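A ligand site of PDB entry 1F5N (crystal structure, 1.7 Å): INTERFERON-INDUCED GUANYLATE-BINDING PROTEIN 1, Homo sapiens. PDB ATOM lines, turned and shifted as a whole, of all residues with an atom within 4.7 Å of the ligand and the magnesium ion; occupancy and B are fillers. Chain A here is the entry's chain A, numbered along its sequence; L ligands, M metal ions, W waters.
OD1 of Asp 184 is in hydrogen-bond range of N4 of the ligand (2.7 Å).
NZ of Lys 51 lies within salt-bridge range of O3 of the ligand (2.7 Å).
An oxygen (O12) of the ligand is in hydrogen-bond range of the backbone carbonyl oxygen (O) of Leu 247, at 2.9 Å.
The backbone NH of Gly 100 lies close to an oxygen (O3) of the ligand, 3.2 Å away.
O8 of the ligand sits at hydrogen-bond distance from N of Gly 68.
The guanidinium group (NH2) of Arg 183 lies within hydrogen-bond range of a nitrogen (N3) of the ligand.
N of Thr 49 sits at hydrogen-bond distance from O4 of the ligand, at 3.0 Å.
The backbone NH (N) of Ser 52 sits at hydrogen-bond distance from an oxygen (O7) of the ligand, at 3.2 Å.
The backbone NH of Tyr 53 is in hydrogen-bond range of an oxygen (O7) of the ligand (2.9 Å).
The backbone NH (N) of His 74 lies within hydrogen-bond range of an oxygen (O1) of the ligand.
The backbone NH (N) of Lys 51 is in hydrogen-bond range of an oxygen (O4) of the ligand, at 2.9 Å.
O2 of the ligand sits close to N of Thr 75 (2.8 Å).
N of Gly 50 sits at hydrogen-bond distance from O4 of the ligand, at 3.1 Å.
OG1 of Thr 49 sits at hydrogen-bond distance from O of Leu 46 (2.7 Å).
The side-chain hydroxyl of Ser 66 lies within hydrogen-bond range of a ring nitrogen (NE2) of His 74.
The side-chain amino group of Lys 51 lies within hydrogen-bond range of the backbone carbonyl oxygen of Leu 46 (3.0 Å).
The guanidinium group (NH1) of Arg 183 lies within hydrogen-bond range of the backbone carbonyl oxygen (O) of Gly 50 (3.0 Å).
The backbone NH (N) of Gln 72 is in hydrogen-bond range of the side-chain hydroxyl (OG) of Ser 69 (3.0 Å).
The side-chain hydroxyl (OG) of Ser 52 sits close to the side-chain carboxylate (OD2) of Asp 97.
NE of Arg 240 lies within salt-bridge range of OD2 of Asp 184.
The backbone carbonyl oxygen (O) of Leu 67 sits close to a ring nitrogen (ND1) of His 74 (3.5 Å).
A nitrogen (N1) of the ligand sits close to the backbone NH (N) of Arg 48 (3.0 Å).
Tyr 47 touches the ligand.
Leu 67 touches the ligand.
O of Ser 69 touches C1 of the ligand, at 3.2 Å.
Thr 70 touches the ligand (OG1 to O11, 3.8 Å).
Ser 73 touches the ligand (CA to O1, 3.3 Å).
Pro 241 touches the ligand (CG to O13, 3.4 Å).
Ala 248 touches the ligand (CA to O11, 3.6 Å).
Leu 250 touches the ligand (CB to O12, 3.4 Å).
Hydrophobic or aromatic side chains that line the ligand: Tyr 47, Tyr 53, Leu 67, His 74, Pro 241, Leu 247 and Leu 250.
Of the 30 residues printed, 21 come within 4 Å of the ligand.
Asp 97 touches the magnesium ion (OD2 to MG, 3.9 Å).
Along chain A the residues within 4 Å of the magnesium ion span positions 52 to 97.
The magnesium ion is bound by water W2 (2.2 Å), O2 of the ligand (2.2 Å), OG1 of Thr 75 (2.2 Å), OG of Ser 52 (2.2 Å), O5 of the ligand (2.2 Å) and water W7 (2.2 Å).
Water W7 bridges O8 of the ligand and O of Ser 66.
Water W2 lies within hydrogen-bond range of O of Thr 98 (2.7 Å) and OD1 of Asp 97 (2.8 Å).
Water W6 lies within hydrogen-bond range of an oxygen (O13) of the ligand (2.6 Å), the backbone NH (N) of Asp 184 (3.0 Å) and the guanidinium group (NE) of Arg 183 (3.5 Å).
Water W9 lies within hydrogen-bond range of O of Thr 75 (2.7 Å), O1 of the ligand (2.7 Å) and N of Gly 100 (3.0 Å).
Water W3 lies within hydrogen-bond range of an oxygen (O12) of the ligand (2.8 Å), the backbone NH of Glu 251 (2.8 Å), the backbone carbonyl oxygen of Ala 248 (3.4 Å) and the backbone NH of Leu 250 (3.4 Å).
Water W1 bridges the backbone carbonyl oxygen (O) of Arg 48 and an oxygen (O10) of the ligand.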
ATOM      1  N   LEU A  46      15.392  -0.778   0.620  1.00  0.00           N
ATOM      2  CA  LEU A  46      14.554  -1.226   1.713  1.00  0.00           C
ATOM      3  C   LEU A  46      13.752  -2.468   1.311  1.00  0.00           C
ATOM      4  O   LEU A  46      13.376  -2.637   0.142  1.00  0.00           O
ATOM      5  CB  LEU A  46      13.604  -0.093   2.123  1.00  0.00           C
ATOM      6  CG  LEU A  46      12.667  -0.305   3.298  1.00  0.00           C
ATOM      7  CD1 LEU A  46      13.489  -0.504   4.573  1.00  0.00           C
ATOM      8  CD2 LEU A  46      11.757   0.895   3.448  1.00  0.00           C
ATOM      9  N   TYR A  47      13.494  -3.353   2.266  1.00  0.00           N
ATOM     10  CA  TYR A  47      12.729  -4.551   1.983  1.00  0.00           C
ATOM     11  C   TYR A  47      11.311  -4.178   1.552  1.00  0.00           C
ATOM     12  O   TYR A  47      10.837  -3.095   1.865  1.00  0.00           O
ATOM     13  CB  TYR A  47      12.693  -5.458   3.233  1.00  0.00           C
ATOM     14  CG  TYR A  47      11.824  -4.954   4.364  1.00  0.00           C
ATOM     15  CD1 TYR A  47      10.539  -5.467   4.561  1.00  0.00           C
ATOM     16  CD2 TYR A  47      12.291  -3.984   5.252  1.00  0.00           C
ATOM     17  CE1 TYR A  47       9.743  -5.035   5.620  1.00  0.00           C
ATOM     18  CE2 TYR A  47      11.502  -3.550   6.318  1.00  0.00           C
ATOM     19  CZ  TYR A  47      10.227  -4.073   6.495  1.00  0.00           C
ATOM     20  OH  TYR A  47       9.448  -3.649   7.542  1.00  0.00           O
ATOM     21  N   ARG A  48      10.667  -5.076   0.822  1.00  0.00           N
ATOM     22  CA  ARG A  48       9.299  -4.877   0.322  1.00  0.00           C
ATOM     23  C   ARG A  48       9.118  -3.665  -0.604  1.00  0.00           C
ATOM     24  O   ARG A  48       8.059  -3.029  -0.587  1.00  0.00           O
ATOM     25  CB  ARG A  48       8.310  -4.776   1.497  1.00  0.00           C
ATOM     26  CG  ARG A  48       8.198  -3.383   2.101  1.00  0.00           C
ATOM     27  CD  ARG A  48       7.297  -3.340   3.321  1.00  0.00           C
ATOM     28  NE  ARG A  48       7.218  -1.995   3.881  1.00  0.00           N
ATOM     29  CZ  ARG A  48       8.264  -1.261   4.244  1.00  0.00           C
ATOM     30  NH1 ARG A  48       9.496  -1.741   4.101  1.00  0.00           N
ATOM     31  NH2 ARG A  48       8.084  -0.054   4.747  1.00  0.00           N
ATOM     32  N   THR A  49      10.134  -3.356  -1.403  1.00  0.00           N
ATOM     33  CA  THR A  49      10.004  -2.226  -2.327  1.00  0.00           C
ATOM     34  C   THR A  49       9.937  -2.654  -3.789  1.00  0.00           C
ATOM     35  O   THR A  49      10.069  -1.817  -4.681  1.00  0.00           O
ATOM     36  CB  THR A  49      11.164  -1.192  -2.152  1.00  0.00           C
ATOM     37  OG1 THR A  49      12.438  -1.849  -2.251  1.00  0.00           O
ATOM     38  CG2 THR A  49      11.040  -0.515  -0.797  1.00  0.00           C
ATOM     39  N   GLY A  50       9.721  -3.941  -4.009  1.00  0.00           N
ATOM     40  CA  GLY A  50       9.615  -4.461  -5.366  1.00  0.00           C
ATOM     41  C   GLY A  50      10.936  -4.660  -6.095  1.00  0.00           C
ATOM     42  O   GLY A  50      10.988  -4.590  -7.332  1.00  0.00           O
ATOM     43  N   LYS A  51      12.007  -4.918  -5.360  1.00  0.00           N
ATOM     44  CA  LYS A  51      13.302  -5.130  -5.986  1.00  0.00           C
ATOM     45  C   LYS A  51      13.343  -6.409  -6.820  1.00  0.00           C
ATOM     46  O   LYS A  51      13.752  -6.396  -7.985  1.00  0.00           O
ATOM     47  CB  LYS A  51      14.406  -5.172  -4.916  1.00  0.00           C
ATOM     48  CG  LYS A  51      14.616  -3.838  -4.238  1.00  0.00           C
ATOM     49  CD  LYS A  51      15.827  -3.878  -3.285  1.00  0.00           C
ATOM     50  CE  LYS A  51      15.686  -5.002  -2.255  1.00  0.00           C
ATOM     51  NZ  LYS A  51      14.432  -4.883  -1.471  1.00  0.00           N
ATOM     52  N   SER A  52      12.942  -7.526  -6.209  1.00  0.00           N
ATOM     53  CA  SER A  52      12.959  -8.805  -6.904  1.00  0.00           C
ATOM     54  C   SER A  52      12.062  -8.754  -8.136  1.00  0.00           C
ATOM     55  O   SER A  52      12.437  -9.251  -9.199  1.00  0.00           O
ATOM     56  CB  SER A  52      12.533  -9.918  -5.956  1.00  0.00           C
ATOM     57  OG  SER A  52      13.556 -10.127  -4.993  1.00  0.00           O
ATOM     58  N   TYR A  53      10.908  -8.126  -7.998  1.00  0.00           N
ATOM     59  CA  TYR A  53       9.964  -8.002  -9.114  1.00  0.00           C
ATOM     60  C   TYR A  53      10.618  -7.279 -10.299  1.00  0.00           C
ATOM     61  O   TYR A  53      10.489  -7.704 -11.458  1.00  0.00           O
ATOM     62  CB  TYR A  53       8.741  -7.209  -8.652  1.00  0.00           C
ATOM     63  CG  TYR A  53       7.744  -6.920  -9.746  1.00  0.00           C
ATOM     64  CD1 TYR A  53       6.903  -7.906 -10.239  1.00  0.00           C
ATOM     65  CD2 TYR A  53       7.632  -5.628 -10.272  1.00  0.00           C
ATOM     66  CE1 TYR A  53       5.966  -7.625 -11.237  1.00  0.00           C
ATOM     67  CE2 TYR A  53       6.700  -5.340 -11.275  1.00  0.00           C
ATOM     68  CZ  TYR A  53       5.874  -6.351 -11.748  1.00  0.00           C
ATOM     69  OH  TYR A  53       4.971  -6.045 -12.741  1.00  0.00           O
ATOM     70  N   SER A  66      12.295 -15.138  -6.314  1.00  0.00           N
ATOM     71  CA  SER A  66      11.038 -15.244  -5.582  1.00  0.00           C
ATOM     72  C   SER A  66      10.591 -13.910  -4.990  1.00  0.00           C
ATOM     73  O   SER A  66      11.418 -13.109  -4.564  1.00  0.00           O
ATOM     74  CB  SER A  66      11.155 -16.293  -4.468  1.00  0.00           C
ATOM     75  OG  SER A  66      12.298 -16.070  -3.675  1.00  0.00           O
ATOM     76  N   LEU A  67       9.285 -13.682  -4.993  1.00  0.00           N
ATOM     77  CA  LEU A  67       8.717 -12.446  -4.462  1.00  0.00           C
ATOM     78  C   LEU A  67       8.101 -12.624  -3.088  1.00  0.00           C
ATOM     79  O   LEU A  67       7.644 -13.716  -2.726  1.00  0.00           O
ATOM     80  CB  LEU A  67       7.643 -11.906  -5.404  1.00  0.00           C
ATOM     81  CG  LEU A  67       7.956 -11.782  -6.897  1.00  0.00           C
ATOM     82  CD1 LEU A  67       6.823 -11.030  -7.571  1.00  0.00           C
ATOM     83  CD2 LEU A  67       9.276 -11.051  -7.092  1.00  0.00           C
ATOM     84  N   GLY A  68       8.076 -11.544  -2.329  1.00  0.00           N
ATOM     85  CA  GLY A  68       7.495 -11.563  -1.004  1.00  0.00           C
ATOM     86  C   GLY A  68       6.186 -10.803  -1.045  1.00  0.00           C
ATOM     87  O   GLY A  68       5.634 -10.573  -2.116  1.00  0.00           O
ATOM     88  N   SER A  69       5.703 -10.411   0.119  1.00  0.00           N
ATOM     89  CA  SER A  69       4.458  -9.660   0.212  1.00  0.00           C
ATOM     90  C   SER A  69       4.800  -8.181   0.324  1.00  0.00           C
ATOM     91  O   SER A  69       5.969  -7.806   0.255  1.00  0.00           O
ATOM     92  CB  SER A  69       3.653 -10.099   1.434  1.00  0.00           C
ATOM     93  OG  SER A  69       4.367  -9.816   2.625  1.00  0.00           O
ATOM     94  N   THR A  70       3.779  -7.357   0.506  1.00  0.00           N
ATOM     95  CA  THR A  70       3.979  -5.915   0.626  1.00  0.00           C
ATOM     96  C   THR A  70       4.266  -5.519   2.070  1.00  0.00           C
ATOM     97  O   THR A  70       4.539  -4.348   2.347  1.00  0.00           O
ATOM     98  CB  THR A  70       2.722  -5.160   0.147  1.00  0.00           C
ATOM     99  OG1 THR A  70       2.454  -5.492  -1.222  1.00  0.00           O
ATOM    100  CG2 THR A  70       2.923  -3.656   0.252  1.00  0.00           C
ATOM    101  N   GLN A  72       6.027  -8.050   4.453  1.00  0.00           N
ATOM    102  CA  GLN A  72       7.056  -8.899   5.065  1.00  0.00           C
ATOM    103  C   GLN A  72       8.284  -9.030   4.172  1.00  0.00           C
ATOM    104  O   GLN A  72       8.169  -9.048   2.950  1.00  0.00           O
ATOM    105  CB  GLN A  72       6.468 -10.296   5.326  1.00  0.00           C
ATOM    106  CG  GLN A  72       7.393 -11.285   6.002  1.00  0.00           C
ATOM    107  CD  GLN A  72       6.704 -12.621   6.281  1.00  0.00           C
ATOM    108  OE1 GLN A  72       5.567 -12.661   6.752  1.00  0.00           O
ATOM    109  NE2 GLN A  72       7.395 -13.730   5.990  1.00  0.00           N
ATOM    110  N   SER A  73       9.469  -9.101   4.784  1.00  0.00           N
ATOM    111  CA  SER A  73      10.710  -9.249   4.043  1.00  0.00           C
ATOM    112  C   SER A  73      10.718 -10.617   3.377  1.00  0.00           C
ATOM    113  O   SER A  73      10.032 -11.536   3.825  1.00  0.00           O
ATOM    114  CB  SER A  73      11.923  -9.132   4.987  1.00  0.00           C
ATOM    115  OG  SER A  73      11.890 -10.131   5.991  1.00  0.00           O
ATOM    116  N   HIS A  74      11.498 -10.771   2.309  1.00  0.00           N
ATOM    117  CA  HIS A  74      11.550 -12.048   1.611  1.00  0.00           C
ATOM    118  C   HIS A  74      12.957 -12.538   1.257  1.00  0.00           C
ATOM    119  O   HIS A  74      13.443 -13.535   1.800  1.00  0.00           O
ATOM    120  CB  HIS A  74      10.701 -11.994   0.338  1.00  0.00           C
ATOM    121  CG  HIS A  74      10.510 -13.323  -0.317  1.00  0.00           C
ATOM    122  ND1 HIS A  74       9.592 -14.251   0.128  1.00  0.00           N
ATOM    123  CD2 HIS A  74      11.164 -13.905  -1.357  1.00  0.00           C
ATOM    124  CE1 HIS A  74       9.677 -15.346  -0.612  1.00  0.00           C
ATOM    125  NE2 HIS A  74      10.632 -15.160  -1.518  1.00  0.00           N
ATOM    126  N   THR A  75      13.628 -11.841   0.341  1.00  0.00           N
ATOM    127  CA  THR A  75      14.954 -12.249  -0.095  1.00  0.00           C
ATOM    128  C   THR A  75      15.998 -12.181   1.014  1.00  0.00           C
ATOM    129  O   THR A  75      16.000 -11.252   1.797  1.00  0.00           O
ATOM    130  CB  THR A  75      15.427 -11.364  -1.269  1.00  0.00           C
ATOM    131  OG1 THR A  75      14.458 -11.439  -2.320  1.00  0.00           O
ATOM    132  CG2 THR A  75      16.772 -11.837  -1.800  1.00  0.00           C
ATOM    133  N   ASP A  97      20.301 -10.039  -6.952  1.00  0.00           N
ATOM    134  CA  ASP A  97      19.169  -9.580  -6.160  1.00  0.00           C
ATOM    135  C   ASP A  97      19.622  -9.667  -4.708  1.00  0.00           C
ATOM    136  O   ASP A  97      20.268 -10.629  -4.319  1.00  0.00           O
ATOM    137  CB  ASP A  97      17.967 -10.501  -6.418  1.00  0.00           C
ATOM    138  CG  ASP A  97      16.713 -10.015  -5.755  1.00  0.00           C
ATOM    139  OD1 ASP A  97      16.629  -8.810  -5.436  1.00  0.00           O
ATOM    140  OD2 ASP A  97      15.786 -10.844  -5.575  1.00  0.00           O
ATOM    141  N   THR A  98      19.286  -8.665  -3.908  1.00  0.00           N
ATOM    142  CA  THR A  98      19.739  -8.650  -2.532  1.00  0.00           C
ATOM    143  C   THR A  98      18.680  -8.576  -1.451  1.00  0.00           C
ATOM    144  O   THR A  98      17.554  -8.134  -1.666  1.00  0.00           O
ATOM    145  CB  THR A  98      20.723  -7.487  -2.291  1.00  0.00           C
ATOM    146  OG1 THR A  98      20.009  -6.240  -2.408  1.00  0.00           O
ATOM    147  CG2 THR A  98      21.847  -7.514  -3.331  1.00  0.00           C
ATOM    148  N   GLU A  99      19.095  -8.997  -0.262  1.00  0.00           N
ATOM    149  CA  GLU A  99      18.256  -8.961   0.934  1.00  0.00           C
ATOM    150  C   GLU A  99      17.897  -7.499   1.186  1.00  0.00           C
ATOM    151  O   GLU A  99      18.765  -6.616   1.176  1.00  0.00           O
ATOM    152  CB  GLU A  99      19.054  -9.507   2.120  1.00  0.00           C
ATOM    153  CG  GLU A  99      18.285  -9.628   3.426  1.00  0.00           C
ATOM    154  CD  GLU A  99      19.100 -10.328   4.500  1.00  0.00           C
ATOM    155  OE1 GLU A  99      19.847 -11.271   4.152  1.00  0.00           O
ATOM    156  OE2 GLU A  99      18.990  -9.944   5.684  1.00  0.00           O
ATOM    157  N   GLY A 100      16.608  -7.261   1.405  1.00  0.00           N
ATOM    158  CA  GLY A 100      16.138  -5.910   1.643  1.00  0.00           C
ATOM    159  C   GLY A 100      16.745  -5.288   2.887  1.00  0.00           C
ATOM    160  O   GLY A 100      16.858  -5.926   3.927  1.00  0.00           O
ATOM    161  N   ARG A 183       9.936   4.135  -6.848  1.00  0.00           N
ATOM    162  CA  ARG A 183       8.666   3.433  -7.018  1.00  0.00           C
ATOM    163  C   ARG A 183       7.459   4.170  -6.463  1.00  0.00           C
ATOM    164  O   ARG A 183       7.582   4.990  -5.558  1.00  0.00           O
ATOM    165  CB  ARG A 183       8.791   2.037  -6.388  1.00  0.00           C
ATOM    166  CG  ARG A 183      10.065   1.293  -6.838  1.00  0.00           C
ATOM    167  CD  ARG A 183      10.006   0.906  -8.317  1.00  0.00           C
ATOM    168  NE  ARG A 183       9.225  -0.314  -8.516  1.00  0.00           N
ATOM    169  CZ  ARG A 183       9.714  -1.546  -8.385  1.00  0.00           C
ATOM    170  NH1 ARG A 183      10.984  -1.725  -8.073  1.00  0.00           N
ATOM    171  NH2 ARG A 183       8.927  -2.596  -8.551  1.00  0.00           N
ATOM    172  N   ASP A 184       6.274   3.890  -7.023  1.00  0.00           N
ATOM    173  CA  ASP A 184       5.032   4.537  -6.605  1.00  0.00           C
ATOM    174  C   ASP A 184       5.240   6.055  -6.548  1.00  0.00           C
ATOM    175  O   ASP A 184       4.721   6.725  -5.641  1.00  0.00           O
ATOM    176  CB  ASP A 184       4.585   4.032  -5.232  1.00  0.00           C
ATOM    177  CG  ASP A 184       4.235   2.551  -5.231  1.00  0.00           C
ATOM    178  OD1 ASP A 184       4.409   1.860  -6.254  1.00  0.00           O
ATOM    179  OD2 ASP A 184       3.766   2.086  -4.166  1.00  0.00           O
ATOM    180  N   ARG A 240       2.558   3.875  -9.585  1.00  0.00           N
ATOM    181  CA  ARG A 240       1.986   2.717  -8.888  1.00  0.00           C
ATOM    182  C   ARG A 240       1.589   1.782 -10.028  1.00  0.00           C
ATOM    183  O   ARG A 240       0.916   2.206 -10.962  1.00  0.00           O
ATOM    184  CB  ARG A 240       0.720   3.125  -8.132  1.00  0.00           C
ATOM    185  CG  ARG A 240       0.918   3.549  -6.699  1.00  0.00           C
ATOM    186  CD  ARG A 240       0.999   2.342  -5.784  1.00  0.00           C
ATOM    187  NE  ARG A 240       1.125   2.741  -4.391  1.00  0.00           N
ATOM    188  CZ  ARG A 240       0.143   3.251  -3.656  1.00  0.00           C
ATOM    189  NH1 ARG A 240      -1.063   3.413  -4.179  1.00  0.00           N
ATOM    190  NH2 ARG A 240       0.371   3.604  -2.405  1.00  0.00           N
ATOM    191  N   PRO A 241       1.983   0.499  -9.953  1.00  0.00           N
ATOM    192  CA  PRO A 241       1.658  -0.469 -11.013  1.00  0.00           C
ATOM    193  C   PRO A 241       0.165  -0.715 -11.204  1.00  0.00           C
ATOM    194  O   PRO A 241      -0.337  -0.744 -12.338  1.00  0.00           O
ATOM    195  CB  PRO A 241       2.350  -1.744 -10.541  1.00  0.00           C
ATOM    196  CG  PRO A 241       3.446  -1.259  -9.661  1.00  0.00           C
ATOM    197  CD  PRO A 241       2.830  -0.114  -8.924  1.00  0.00           C
ATOM    198  N   LEU A 247      -1.916  -5.064  -5.902  1.00  0.00           N
ATOM    199  CA  LEU A 247      -0.464  -5.043  -5.798  1.00  0.00           C
ATOM    200  C   LEU A 247       0.144  -6.409  -5.487  1.00  0.00           C
ATOM    201  O   LEU A 247       1.186  -6.776  -6.039  1.00  0.00           O
ATOM    202  CB  LEU A 247      -0.016  -4.026  -4.747  1.00  0.00           C
ATOM    203  CG  LEU A 247      -0.217  -2.549  -5.118  1.00  0.00           C
ATOM    204  CD1 LEU A 247       0.053  -1.662  -3.916  1.00  0.00           C
ATOM    205  CD2 LEU A 247       0.726  -2.196  -6.264  1.00  0.00           C
ATOM    206  N   ALA A 248      -0.510  -7.168  -4.612  1.00  0.00           N
ATOM    207  CA  ALA A 248      -0.013  -8.485  -4.218  1.00  0.00           C
ATOM    208  C   ALA A 248      -0.119  -9.564  -5.304  1.00  0.00           C
ATOM    209  O   ALA A 248       0.465 -10.638  -5.171  1.00  0.00           O
ATOM    210  CB  ALA A 248      -0.750  -8.956  -2.955  1.00  0.00           C
ATOM    211  N   LEU A 250       0.460  -8.687  -8.590  1.00  0.00           N
ATOM    212  CA  LEU A 250       1.217  -8.123  -9.693  1.00  0.00           C
ATOM    213  C   LEU A 250       1.948  -9.140 -10.567  1.00  0.00           C
ATOM    214  O   LEU A 250       1.852  -9.099 -11.793  1.00  0.00           O
ATOM    215  CB  LEU A 250       2.215  -7.097  -9.156  1.00  0.00           C
ATOM    216  CG  LEU A 250       2.829  -6.118 -10.165  1.00  0.00           C
ATOM    217  CD1 LEU A 250       1.720  -5.374 -10.898  1.00  0.00           C
ATOM    218  CD2 LEU A 250       3.736  -5.146  -9.434  1.00  0.00           C
ATOM    219  N   GLU A 251       2.664 -10.063  -9.929  1.00  0.00           N
ATOM    220  CA  GLU A 251       3.426 -11.073 -10.645  1.00  0.00           C
ATOM    221  C   GLU A 251       2.592 -11.922 -11.611  1.00  0.00           C
ATOM    222  O   GLU A 251       3.081 -12.350 -12.652  1.00  0.00           O
ATOM    223  CB  GLU A 251       4.131 -11.984  -9.630  1.00  0.00           C
ATOM    224  CG  GLU A 251       4.935 -13.111 -10.251  1.00  0.00           C
ATOM    225  CD  GLU A 251       5.918 -13.730  -9.268  1.00  0.00           C
ATOM    226  OE1 GLU A 251       5.490 -14.150  -8.169  1.00  0.00           O
ATOM    227  OE2 GLU A 251       7.125 -13.805  -9.600  1.00  0.00           O
ATOM    228  N   PHE A 262       3.421   2.722 -16.281  1.00  0.00           N
ATOM    229  CA  PHE A 262       4.346   1.902 -15.496  1.00  0.00           C
ATOM    230  C   PHE A 262       5.000   0.881 -16.410  1.00  0.00           C
ATOM    231  O   PHE A 262       6.207   0.641 -16.348  1.00  0.00           O
ATOM    232  CB  PHE A 262       3.602   1.148 -14.375  1.00  0.00           C
ATOM    233  CG  PHE A 262       4.462   0.141 -13.653  1.00  0.00           C
ATOM    234  CD1 PHE A 262       5.399   0.563 -12.705  1.00  0.00           C
ATOM    235  CD2 PHE A 262       4.345  -1.211 -13.915  1.00  0.00           C
ATOM    236  CE1 PHE A 262       6.198  -0.372 -12.042  1.00  0.00           C
ATOM    237  CE2 PHE A 262       5.139  -2.148 -13.260  1.00  0.00           C
ATOM    238  CZ  PHE A 262       6.075  -1.726 -12.311  1.00  0.00           C
HETATM  239  P1  LIG L   1      12.651  -8.059  -0.067  1.00  0.00           P
HETATM  240  O1  LIG L   1      12.354  -8.305   1.334  1.00  0.00           O
HETATM  241  O2  LIG L   1      13.182  -9.252  -0.669  1.00  0.00           O
HETATM  242  O3  LIG L   1      13.821  -7.070  -0.076  1.00  0.00           O
HETATM  243  N1  LIG L   1      11.389  -7.411  -0.889  1.00  0.00           N
HETATM  244  P2  LIG L   1      11.514  -6.861  -2.425  1.00  0.00           P
HETATM  245  O4  LIG L   1      11.940  -5.458  -2.538  1.00  0.00           O
HETATM  246  O5  LIG L   1      12.219  -7.740  -3.321  1.00  0.00           O
HETATM  247  O6  LIG L   1      10.007  -6.869  -2.987  1.00  0.00           O
HETATM  248  P3  LIG L   1       9.333  -7.952  -3.995  1.00  0.00           P
HETATM  249  O7  LIG L   1       9.885  -7.761  -5.359  1.00  0.00           O
HETATM  250  O8  LIG L   1       9.413  -9.313  -3.402  1.00  0.00           O
HETATM  251  O9  LIG L   1       7.805  -7.448  -3.979  1.00  0.00           O
HETATM  252  C1  LIG L   1       7.063  -7.412  -2.732  1.00  0.00           C
HETATM  253  C2  LIG L   1       5.588  -7.055  -3.019  1.00  0.00           C
HETATM  254  O10 LIG L   1       5.512  -5.741  -3.592  1.00  0.00           O
HETATM  255  C3  LIG L   1       4.892  -8.014  -4.009  1.00  0.00           C
HETATM  256  O11 LIG L   1       3.517  -8.193  -3.626  1.00  0.00           O
HETATM  257  C4  LIG L   1       4.997  -7.231  -5.343  1.00  0.00           C
HETATM  258  O12 LIG L   1       3.933  -7.574  -6.241  1.00  0.00           O
HETATM  259  C5  LIG L   1       4.805  -5.802  -4.839  1.00  0.00           C
HETATM  260  N2  LIG L   1       5.365  -4.801  -5.782  1.00  0.00           N
HETATM  261  C6  LIG L   1       6.230  -4.946  -6.870  1.00  0.00           C
HETATM  262  N3  LIG L   1       6.516  -3.851  -7.485  1.00  0.00           N
HETATM  263  C7  LIG L   1       5.814  -2.874  -6.772  1.00  0.00           C
HETATM  264  C8  LIG L   1       5.699  -1.426  -6.958  1.00  0.00           C
HETATM  265  O13 LIG L   1       6.228  -0.725  -7.835  1.00  0.00           O
HETATM  266  N4  LIG L   1       4.880  -0.818  -5.999  1.00  0.00           N
HETATM  267  C9  LIG L   1       4.275  -1.457  -4.940  1.00  0.00           C
HETATM  268  N5  LIG L   1       3.578  -0.736  -4.042  1.00  0.00           N
HETATM  269  N6  LIG L   1       4.368  -2.823  -4.766  1.00  0.00           N
HETATM  270  C10 LIG L   1       5.125  -3.447  -5.710  1.00  0.00           C
HETATM  271 MG    MG M   1      13.376  -9.581  -2.848  1.00  0.00          MG
HETATM  272  O   HOH W   1       5.464  -3.284  -1.639  1.00  0.00           O
HETATM  273  O   HOH W   2      15.265  -8.507  -3.027  1.00  0.00           O
HETATM  274  O   HOH W   3       3.221 -10.165  -7.145  1.00  0.00           O
HETATM  275  O   HOH W   4       3.538  -1.067  -1.183  1.00  0.00           O
HETATM  276  O   HOH W   5       8.773  -8.528   0.226  1.00  0.00           O
HETATM  277  O   HOH W   6       6.398   1.664  -8.959  1.00  0.00           O
HETATM  278  O   HOH W   7      11.495 -10.806  -2.893  1.00  0.00           O
HETATM  279  O   HOH W   8       3.197 -11.083  -3.680  1.00  0.00           O
HETATM  280  O   HOH W   9      14.598  -9.106   2.651  1.00  0.00           O
